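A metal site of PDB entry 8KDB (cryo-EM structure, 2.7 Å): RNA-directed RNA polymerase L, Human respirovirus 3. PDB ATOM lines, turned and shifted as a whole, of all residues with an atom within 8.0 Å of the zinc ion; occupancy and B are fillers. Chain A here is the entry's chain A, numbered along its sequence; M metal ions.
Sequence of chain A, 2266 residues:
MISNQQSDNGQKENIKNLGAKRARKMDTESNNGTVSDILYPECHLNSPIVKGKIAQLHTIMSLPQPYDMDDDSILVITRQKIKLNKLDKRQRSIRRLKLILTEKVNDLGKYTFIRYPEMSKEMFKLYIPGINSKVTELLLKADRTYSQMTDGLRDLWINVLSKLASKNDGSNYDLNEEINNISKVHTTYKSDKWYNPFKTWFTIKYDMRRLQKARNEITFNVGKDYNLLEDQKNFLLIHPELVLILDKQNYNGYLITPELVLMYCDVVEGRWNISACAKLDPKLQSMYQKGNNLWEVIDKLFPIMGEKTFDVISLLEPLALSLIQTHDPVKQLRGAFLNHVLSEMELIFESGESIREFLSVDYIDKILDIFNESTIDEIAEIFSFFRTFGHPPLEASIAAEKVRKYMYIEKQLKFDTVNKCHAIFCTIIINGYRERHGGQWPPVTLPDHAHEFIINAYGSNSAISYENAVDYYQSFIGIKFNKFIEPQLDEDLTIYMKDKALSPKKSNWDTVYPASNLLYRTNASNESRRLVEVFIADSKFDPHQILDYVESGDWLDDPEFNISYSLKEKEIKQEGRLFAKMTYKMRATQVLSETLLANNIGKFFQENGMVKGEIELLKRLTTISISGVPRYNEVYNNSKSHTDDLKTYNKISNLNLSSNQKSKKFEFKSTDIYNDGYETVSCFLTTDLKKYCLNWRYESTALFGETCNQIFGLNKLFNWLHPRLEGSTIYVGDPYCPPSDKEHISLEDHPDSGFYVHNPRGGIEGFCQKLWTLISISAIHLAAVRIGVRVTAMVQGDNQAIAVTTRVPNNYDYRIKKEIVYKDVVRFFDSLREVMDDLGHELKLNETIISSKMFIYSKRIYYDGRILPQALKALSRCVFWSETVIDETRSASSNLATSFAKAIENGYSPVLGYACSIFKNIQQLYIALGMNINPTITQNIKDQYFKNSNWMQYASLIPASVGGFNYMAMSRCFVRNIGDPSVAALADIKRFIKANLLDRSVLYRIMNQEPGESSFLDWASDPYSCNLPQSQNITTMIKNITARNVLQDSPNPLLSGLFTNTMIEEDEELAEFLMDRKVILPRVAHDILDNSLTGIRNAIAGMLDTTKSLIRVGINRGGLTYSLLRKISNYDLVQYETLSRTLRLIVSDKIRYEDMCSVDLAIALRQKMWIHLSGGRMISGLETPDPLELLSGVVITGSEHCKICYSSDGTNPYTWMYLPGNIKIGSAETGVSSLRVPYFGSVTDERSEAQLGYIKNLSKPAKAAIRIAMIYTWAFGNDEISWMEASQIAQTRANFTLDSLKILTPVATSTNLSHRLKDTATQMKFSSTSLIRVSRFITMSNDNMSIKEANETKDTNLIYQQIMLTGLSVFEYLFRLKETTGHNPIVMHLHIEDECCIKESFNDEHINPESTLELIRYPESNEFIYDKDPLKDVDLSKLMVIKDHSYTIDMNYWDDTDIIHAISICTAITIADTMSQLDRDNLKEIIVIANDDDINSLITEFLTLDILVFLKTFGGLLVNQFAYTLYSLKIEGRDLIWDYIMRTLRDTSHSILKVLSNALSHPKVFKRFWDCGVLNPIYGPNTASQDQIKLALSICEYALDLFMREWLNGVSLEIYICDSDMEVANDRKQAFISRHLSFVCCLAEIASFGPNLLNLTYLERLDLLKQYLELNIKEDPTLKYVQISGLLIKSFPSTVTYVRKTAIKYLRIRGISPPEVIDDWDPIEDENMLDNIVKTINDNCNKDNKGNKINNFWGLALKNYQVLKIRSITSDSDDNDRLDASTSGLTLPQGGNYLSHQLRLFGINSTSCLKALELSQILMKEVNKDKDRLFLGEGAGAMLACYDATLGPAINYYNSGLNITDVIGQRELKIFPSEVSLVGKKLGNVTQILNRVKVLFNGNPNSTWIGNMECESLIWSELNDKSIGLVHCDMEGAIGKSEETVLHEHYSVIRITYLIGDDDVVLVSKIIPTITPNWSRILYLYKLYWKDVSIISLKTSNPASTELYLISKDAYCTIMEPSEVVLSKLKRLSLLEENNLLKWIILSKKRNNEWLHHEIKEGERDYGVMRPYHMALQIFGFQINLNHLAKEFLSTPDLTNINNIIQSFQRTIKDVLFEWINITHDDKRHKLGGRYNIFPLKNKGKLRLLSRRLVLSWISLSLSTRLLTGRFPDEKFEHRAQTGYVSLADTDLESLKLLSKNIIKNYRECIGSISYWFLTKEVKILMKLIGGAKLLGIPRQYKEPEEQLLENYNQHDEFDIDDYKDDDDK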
ATOM      1  N   SER A1192       4.421  13.792  26.883  1.00  0.00           N
ATOM      2  CA  SER A1192       5.773  14.165  26.484  1.00  0.00           C
ATOM      3  C   SER A1192       6.233  15.258  27.438  1.00  0.00           C
ATOM      4  O   SER A1192       5.675  16.360  27.432  1.00  0.00           O
ATOM      5  CB  SER A1192       5.813  14.649  25.042  1.00  0.00           C
ATOM      6  OG  SER A1192       5.529  13.598  24.137  1.00  0.00           O
ATOM      7  N   GLY A1193       7.220  14.958  28.263  1.00  0.00           N
ATOM      8  CA  GLY A1193       7.709  15.897  29.269  1.00  0.00           C
ATOM      9  C   GLY A1193       8.967  16.603  28.816  1.00  0.00           C
ATOM     10  O   GLY A1193       9.883  15.979  28.290  1.00  0.00           O
ATOM     11  N   VAL A1194       8.997  17.922  29.026  1.00  0.00           N
ATOM     12  CA  VAL A1194      10.142  18.749  28.679  1.00  0.00           C
ATOM     13  C   VAL A1194      10.571  19.504  29.921  1.00  0.00           C
ATOM     14  O   VAL A1194       9.767  20.204  30.541  1.00  0.00           O
ATOM     15  CB  VAL A1194       9.824  19.734  27.534  1.00  0.00           C
ATOM     16  CG1 VAL A1194      11.010  20.634  27.270  1.00  0.00           C
ATOM     17  CG2 VAL A1194       9.438  18.979  26.283  1.00  0.00           C
ATOM     18  N   ILE A1196      12.541  22.491  31.140  1.00  0.00           N
ATOM     19  CA  ILE A1196      13.038  23.735  30.577  1.00  0.00           C
ATOM     20  C   ILE A1196      14.163  24.265  31.465  1.00  0.00           C
ATOM     21  O   ILE A1196      13.990  24.423  32.673  1.00  0.00           O
ATOM     22  CB  ILE A1196      11.913  24.775  30.454  1.00  0.00           C
ATOM     23  CG1 ILE A1196      10.998  24.418  29.280  1.00  0.00           C
ATOM     24  CG2 ILE A1196      12.477  26.172  30.285  1.00  0.00           C
ATOM     25  CD1 ILE A1196       9.597  24.938  29.419  1.00  0.00           C
ATOM     26  N   HIS A1201      13.913  27.898  24.703  1.00  0.00           N
ATOM     27  CA  HIS A1201      12.466  27.754  24.621  1.00  0.00           C
ATOM     28  C   HIS A1201      12.073  26.282  24.558  1.00  0.00           C
ATOM     29  O   HIS A1201      12.853  25.419  24.171  1.00  0.00           O
ATOM     30  CB  HIS A1201      11.919  28.501  23.408  1.00  0.00           C
ATOM     31  CG  HIS A1201      11.778  29.975  23.611  1.00  0.00           C
ATOM     32  ND1 HIS A1201      10.727  30.517  24.315  1.00  0.00           N
ATOM     33  CD2 HIS A1201      12.536  31.014  23.196  1.00  0.00           C
ATOM     34  CE1 HIS A1201      10.854  31.834  24.337  1.00  0.00           C
ATOM     35  NE2 HIS A1201      11.946  32.155  23.663  1.00  0.00           N
ATOM     36  N   CYS A1202      10.836  26.014  24.968  1.00  0.00           N
ATOM     37  CA  CYS A1202      10.279  24.673  24.858  1.00  0.00           C
ATOM     38  C   CYS A1202      10.178  24.272  23.388  1.00  0.00           C
ATOM     39  O   CYS A1202       9.556  24.968  22.581  1.00  0.00           O
ATOM     40  CB  CYS A1202       8.905  24.614  25.517  1.00  0.00           C
ATOM     41  SG  CYS A1202       8.090  22.999  25.454  1.00  0.00           S
ATOM     42  N   LYS A1203      10.814  23.149  23.049  1.00  0.00           N
ATOM     43  CA  LYS A1203      10.835  22.719  21.643  1.00  0.00           C
ATOM     44  C   LYS A1203       9.432  22.393  21.151  1.00  0.00           C
ATOM     45  O   LYS A1203       9.078  22.743  20.015  1.00  0.00           O
ATOM     46  CB  LYS A1203      11.764  21.517  21.485  1.00  0.00           C
ATOM     47  CG  LYS A1203      11.429  20.317  22.361  1.00  0.00           C
ATOM     48  CD  LYS A1203      12.467  19.219  22.205  1.00  0.00           C
ATOM     49  CE  LYS A1203      12.108  18.004  23.050  1.00  0.00           C
ATOM     50  NZ  LYS A1203      13.122  16.928  22.910  1.00  0.00           N
ATOM     51  N   ILE A1204       8.620  21.747  21.978  1.00  0.00           N
ATOM     52  CA  ILE A1204       7.258  21.401  21.558  1.00  0.00           C
ATOM     53  C   ILE A1204       6.392  22.642  21.448  1.00  0.00           C
ATOM     54  O   ILE A1204       5.576  22.774  20.531  1.00  0.00           O
ATOM     55  CB  ILE A1204       6.652  20.366  22.527  1.00  0.00           C
ATOM     56  CG1 ILE A1204       7.510  19.093  22.546  1.00  0.00           C
ATOM     57  CG2 ILE A1204       5.232  20.019  22.114  1.00  0.00           C
ATOM     58  CD1 ILE A1204       7.129  18.120  23.625  1.00  0.00           C
ATOM     59  N   CYS A1205       6.554  23.592  22.384  1.00  0.00           N
ATOM     60  CA  CYS A1205       5.791  24.831  22.310  1.00  0.00           C
ATOM     61  C   CYS A1205       6.204  25.658  21.102  1.00  0.00           C
ATOM     62  O   CYS A1205       5.371  26.321  20.485  1.00  0.00           O
ATOM     63  CB  CYS A1205       5.969  25.634  23.597  1.00  0.00           C
ATOM     64  SG  CYS A1205       5.145  24.956  25.045  1.00  0.00           S
ATOM     65  N   TYR A1206       7.495  25.643  20.757  1.00  0.00           N
ATOM     66  CA  TYR A1206       7.966  26.420  19.614  1.00  0.00           C
ATOM     67  C   TYR A1206       7.526  25.796  18.296  1.00  0.00           C
ATOM     68  O   TYR A1206       7.113  26.503  17.366  1.00  0.00           O
ATOM     69  CB  TYR A1206       9.482  26.571  19.654  1.00  0.00           C
ATOM     70  CG  TYR A1206      10.053  27.187  18.409  1.00  0.00           C
ATOM     71  CD1 TYR A1206       9.664  28.454  17.996  1.00  0.00           C
ATOM     72  CD2 TYR A1206      10.972  26.500  17.624  1.00  0.00           C
ATOM     73  CE1 TYR A1206      10.180  29.020  16.850  1.00  0.00           C
ATOM     74  CE2 TYR A1206      11.497  27.056  16.473  1.00  0.00           C
ATOM     75  CZ  TYR A1206      11.096  28.317  16.096  1.00  0.00           C
ATOM     76  OH  TYR A1206      11.613  28.883  14.949  1.00  0.00           O
ATOM     77  N   SER A1208       4.926  23.885  17.596  1.00  0.00           N
ATOM     78  CA  SER A1208       3.489  24.029  17.401  1.00  0.00           C
ATOM     79  C   SER A1208       3.017  25.473  17.531  1.00  0.00           C
ATOM     80  O   SER A1208       1.816  25.722  17.394  1.00  0.00           O
ATOM     81  CB  SER A1208       2.734  23.156  18.408  1.00  0.00           C
ATOM     82  OG  SER A1208       3.239  23.337  19.717  1.00  0.00           O
ATOM     83  N   GLY A1210       2.717  27.276  20.131  1.00  0.00           N
ATOM     84  CA  GLY A1210       1.928  27.475  21.332  1.00  0.00           C
ATOM     85  C   GLY A1210       0.515  26.934  21.297  1.00  0.00           C
ATOM     86  O   GLY A1210      -0.267  27.257  22.196  1.00  0.00           O
ATOM     87  N   ASN A1212      -0.185  23.647  21.383  1.00  0.00           N
ATOM     88  CA  ASN A1212      -0.213  22.332  21.993  1.00  0.00           C
ATOM     89  C   ASN A1212      -0.503  22.461  23.483  1.00  0.00           C
ATOM     90  O   ASN A1212       0.246  23.148  24.190  1.00  0.00           O
ATOM     91  CB  ASN A1212       1.119  21.620  21.796  1.00  0.00           C
ATOM     92  CG  ASN A1212       1.006  20.123  21.942  1.00  0.00           C
ATOM     93  OD1 ASN A1212       0.525  19.613  22.964  1.00  0.00           O
ATOM     94  ND2 ASN A1212       1.451  19.393  20.929  1.00  0.00           N
ATOM     95  N   PRO A1213      -1.573  21.858  23.994  1.00  0.00           N
ATOM     96  CA  PRO A1213      -1.874  21.969  25.419  1.00  0.00           C
ATOM     97  C   PRO A1213      -0.822  21.281  26.266  1.00  0.00           C
ATOM     98  O   PRO A1213      -0.175  20.319  25.843  1.00  0.00           O
ATOM     99  CB  PRO A1213      -3.232  21.270  25.555  1.00  0.00           C
ATOM    100  CG  PRO A1213      -3.319  20.381  24.363  1.00  0.00           C
ATOM    101  CD  PRO A1213      -2.586  21.070  23.261  1.00  0.00           C
ATOM    102  N   TYR A1214      -0.650  21.784  27.488  1.00  0.00           N
ATOM    103  CA  TYR A1214       0.332  21.203  28.398  1.00  0.00           C
ATOM    104  C   TYR A1214      -0.025  21.565  29.828  1.00  0.00           C
ATOM    105  O   TYR A1214      -0.770  22.513  30.087  1.00  0.00           O
ATOM    106  CB  TYR A1214       1.747  21.688  28.073  1.00  0.00           C
ATOM    107  CG  TYR A1214       1.962  23.167  28.233  1.00  0.00           C
ATOM    108  CD1 TYR A1214       1.530  24.061  27.277  1.00  0.00           C
ATOM    109  CD2 TYR A1214       2.590  23.672  29.362  1.00  0.00           C
ATOM    110  CE1 TYR A1214       1.724  25.417  27.420  1.00  0.00           C
ATOM    111  CE2 TYR A1214       2.783  25.028  29.518  1.00  0.00           C
ATOM    112  CZ  TYR A1214       2.353  25.901  28.551  1.00  0.00           C
ATOM    113  OH  TYR A1214       2.540  27.247  28.701  1.00  0.00           O
ATOM    114  N   THR A1215       0.542  20.791  30.752  1.00  0.00           N
ATOM    115  CA  THR A1215       0.454  21.061  32.182  1.00  0.00           C
ATOM    116  C   THR A1215       1.776  21.655  32.658  1.00  0.00           C
ATOM    117  O   THR A1215       2.852  21.183  32.265  1.00  0.00           O
ATOM    118  CB  THR A1215       0.129  19.778  32.961  1.00  0.00           C
ATOM    119  OG1 THR A1215      -1.212  19.369  32.675  1.00  0.00           O
ATOM    120  CG2 THR A1215       0.255  20.012  34.462  1.00  0.00           C
ATOM    121  N   TRP A1216       1.699  22.685  33.485  1.00  0.00           N
ATOM    122  CA  TRP A1216       2.885  23.439  33.901  1.00  0.00           C
ATOM    123  C   TRP A1216       3.265  23.056  35.326  1.00  0.00           C
ATOM    124  O   TRP A1216       2.406  23.052  36.218  1.00  0.00           O
ATOM    125  CB  TRP A1216       2.606  24.940  33.800  1.00  0.00           C
ATOM    126  CG  TRP A1216       3.715  25.819  34.268  1.00  0.00           C
ATOM    127  CD1 TRP A1216       4.788  26.244  33.542  1.00  0.00           C
ATOM    128  CD2 TRP A1216       3.851  26.412  35.568  1.00  0.00           C
ATOM    129  NE1 TRP A1216       5.586  27.052  34.321  1.00  0.00           N
ATOM    130  CE2 TRP A1216       5.031  27.172  35.558  1.00  0.00           C
ATOM    131  CE3 TRP A1216       3.086  26.355  36.739  1.00  0.00           C
ATOM    132  CZ2 TRP A1216       5.474  27.871  36.672  1.00  0.00           C
ATOM    133  CZ3 TRP A1216       3.530  27.063  37.838  1.00  0.00           C
ATOM    134  CH2 TRP A1216       4.700  27.809  37.799  1.00  0.00           C
ATOM    135  N   MET A1388       8.789  22.412  34.189  1.00  0.00           N
ATOM    136  CA  MET A1388       8.454  21.293  33.321  1.00  0.00           C
ATOM    137  C   MET A1388       7.149  21.555  32.591  1.00  0.00           C
ATOM    138  O   MET A1388       6.165  22.025  33.191  1.00  0.00           O
ATOM    139  CB  MET A1388       8.342  19.979  34.120  1.00  0.00           C
ATOM    140  CG  MET A1388       8.106  18.762  33.242  1.00  0.00           C
ATOM    141  SD  MET A1388       7.993  17.223  34.177  1.00  0.00           S
ATOM    142  CE  MET A1388       9.701  16.994  34.673  1.00  0.00           C
ATOM    143  N   HIS A1389       7.148  21.260  31.296  1.00  0.00           N
ATOM    144  CA  HIS A1389       5.940  21.240  30.470  1.00  0.00           C
ATOM    145  C   HIS A1389       5.571  19.799  30.169  1.00  0.00           C
ATOM    146  O   HIS A1389       6.388  19.040  29.638  1.00  0.00           O
ATOM    147  CB  HIS A1389       6.140  22.009  29.167  1.00  0.00           C
ATOM    148  CG  HIS A1389       6.219  23.494  29.328  1.00  0.00           C
ATOM    149  ND1 HIS A1389       6.203  24.357  28.263  1.00  0.00           N
ATOM    150  CD2 HIS A1389       6.301  24.262  30.440  1.00  0.00           C
ATOM    151  CE1 HIS A1389       6.284  25.604  28.697  1.00  0.00           C
ATOM    152  NE2 HIS A1389       6.347  25.572  30.020  1.00  0.00           N
ATOM    153  N   LEU A1390       4.337  19.420  30.492  1.00  0.00           N
ATOM    154  CA  LEU A1390       3.807  18.094  30.183  1.00  0.00           C
ATOM    155  C   LEU A1390       2.837  18.251  29.024  1.00  0.00           C
ATOM    156  O   LEU A1390       1.667  18.592  29.204  1.00  0.00           O
ATOM    157  CB  LEU A1390       3.138  17.484  31.413  1.00  0.00           C
ATOM    158  CG  LEU A1390       4.027  17.136  32.598  1.00  0.00           C
ATOM    159  CD1 LEU A1390       3.166  16.871  33.809  1.00  0.00           C
ATOM    160  CD2 LEU A1390       4.880  15.920  32.272  1.00  0.00           C
ATOM    161  N   HIS A1391       3.341  18.052  27.811  1.00  0.00           N
ATOM    162  CA  HIS A1391       2.521  18.150  26.624  1.00  0.00           C
ATOM    163  C   HIS A1391       1.877  16.800  26.316  1.00  0.00           C
ATOM    164  O   HIS A1391       2.292  15.758  26.826  1.00  0.00           O
ATOM    165  CB  HIS A1391       3.357  18.598  25.430  1.00  0.00           C
ATOM    166  CG  HIS A1391       3.787  20.041  25.495  1.00  0.00           C
ATOM    167  ND1 HIS A1391       3.060  21.056  24.921  1.00  0.00           N
ATOM    168  CD2 HIS A1391       4.859  20.621  26.074  1.00  0.00           C
ATOM    169  CE1 HIS A1391       3.670  22.210  25.133  1.00  0.00           C
ATOM    170  NE2 HIS A1391       4.764  21.968  25.831  1.00  0.00           N
ATOM    171  N   GLU A1868       0.298  29.624  36.292  1.00  0.00           N
ATOM    172  CA  GLU A1868       1.615  29.594  35.664  1.00  0.00           C
ATOM    173  C   GLU A1868       2.275  30.965  35.742  1.00  0.00           C
ATOM    174  O   GLU A1868       1.598  31.990  35.635  1.00  0.00           O
ATOM    175  CB  GLU A1868       1.494  29.143  34.205  1.00  0.00           C
ATOM    176  CG  GLU A1868       2.756  29.299  33.388  1.00  0.00           C
ATOM    177  CD  GLU A1868       2.589  28.860  31.950  1.00  0.00           C
ATOM    178  OE1 GLU A1868       1.524  28.284  31.631  1.00  0.00           O
ATOM    179  OE2 GLU A1868       3.511  29.088  31.141  1.00  0.00           O
ATOM    180  N   ASN A1898      11.158  32.727  28.841  1.00  0.00           N
ATOM    181  CA  ASN A1898      11.006  31.344  28.391  1.00  0.00           C
ATOM    182  C   ASN A1898      10.335  30.447  29.426  1.00  0.00           C
ATOM    183  O   ASN A1898      10.244  29.236  29.209  1.00  0.00           O
ATOM    184  CB  ASN A1898      12.360  30.760  27.994  1.00  0.00           C
ATOM    185  CG  ASN A1898      13.215  30.381  29.185  1.00  0.00           C
ATOM    186  OD1 ASN A1898      13.046  30.909  30.283  1.00  0.00           O
ATOM    187  ND2 ASN A1898      14.138  29.455  28.977  1.00  0.00           N
HETATM  188 ZN    ZN M   1       6.067  23.418  26.459  1.00  0.00          ZN
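The zinc ion is bound by a ring nitrogen (ND1) of His 1389, a ring nitrogen (NE2) of His 1391, the side-chain sulfur (SG) of Cys 1205 and the side-chain sulfur (SG) of Cys 1202.
The backbone NH (N) of Ile 1204 lies close to the side-chain sulfur (SG) of Cys 1202, at 3.7 Å.
O of Cys 1205 is in hydrogen-bond range of N of Gly 1210.
N of Ser 1192 sits at hydrogen-bond distance from O of His 1391, 2.9 Å away.
The backbone NH (N) of Val 1194 lies within hydrogen-bond range of the backbone carbonyl oxygen (O) of His 1389 (2.9 Å).
A ring nitrogen (ND1) of His 1391 lies within hydrogen-bond range of the backbone carbonyl oxygen (O) of Pro 1213 (3.4 Å).
The nearest printed residue that does not touch the zinc ion is Tyr 1214 (4.5 Å).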
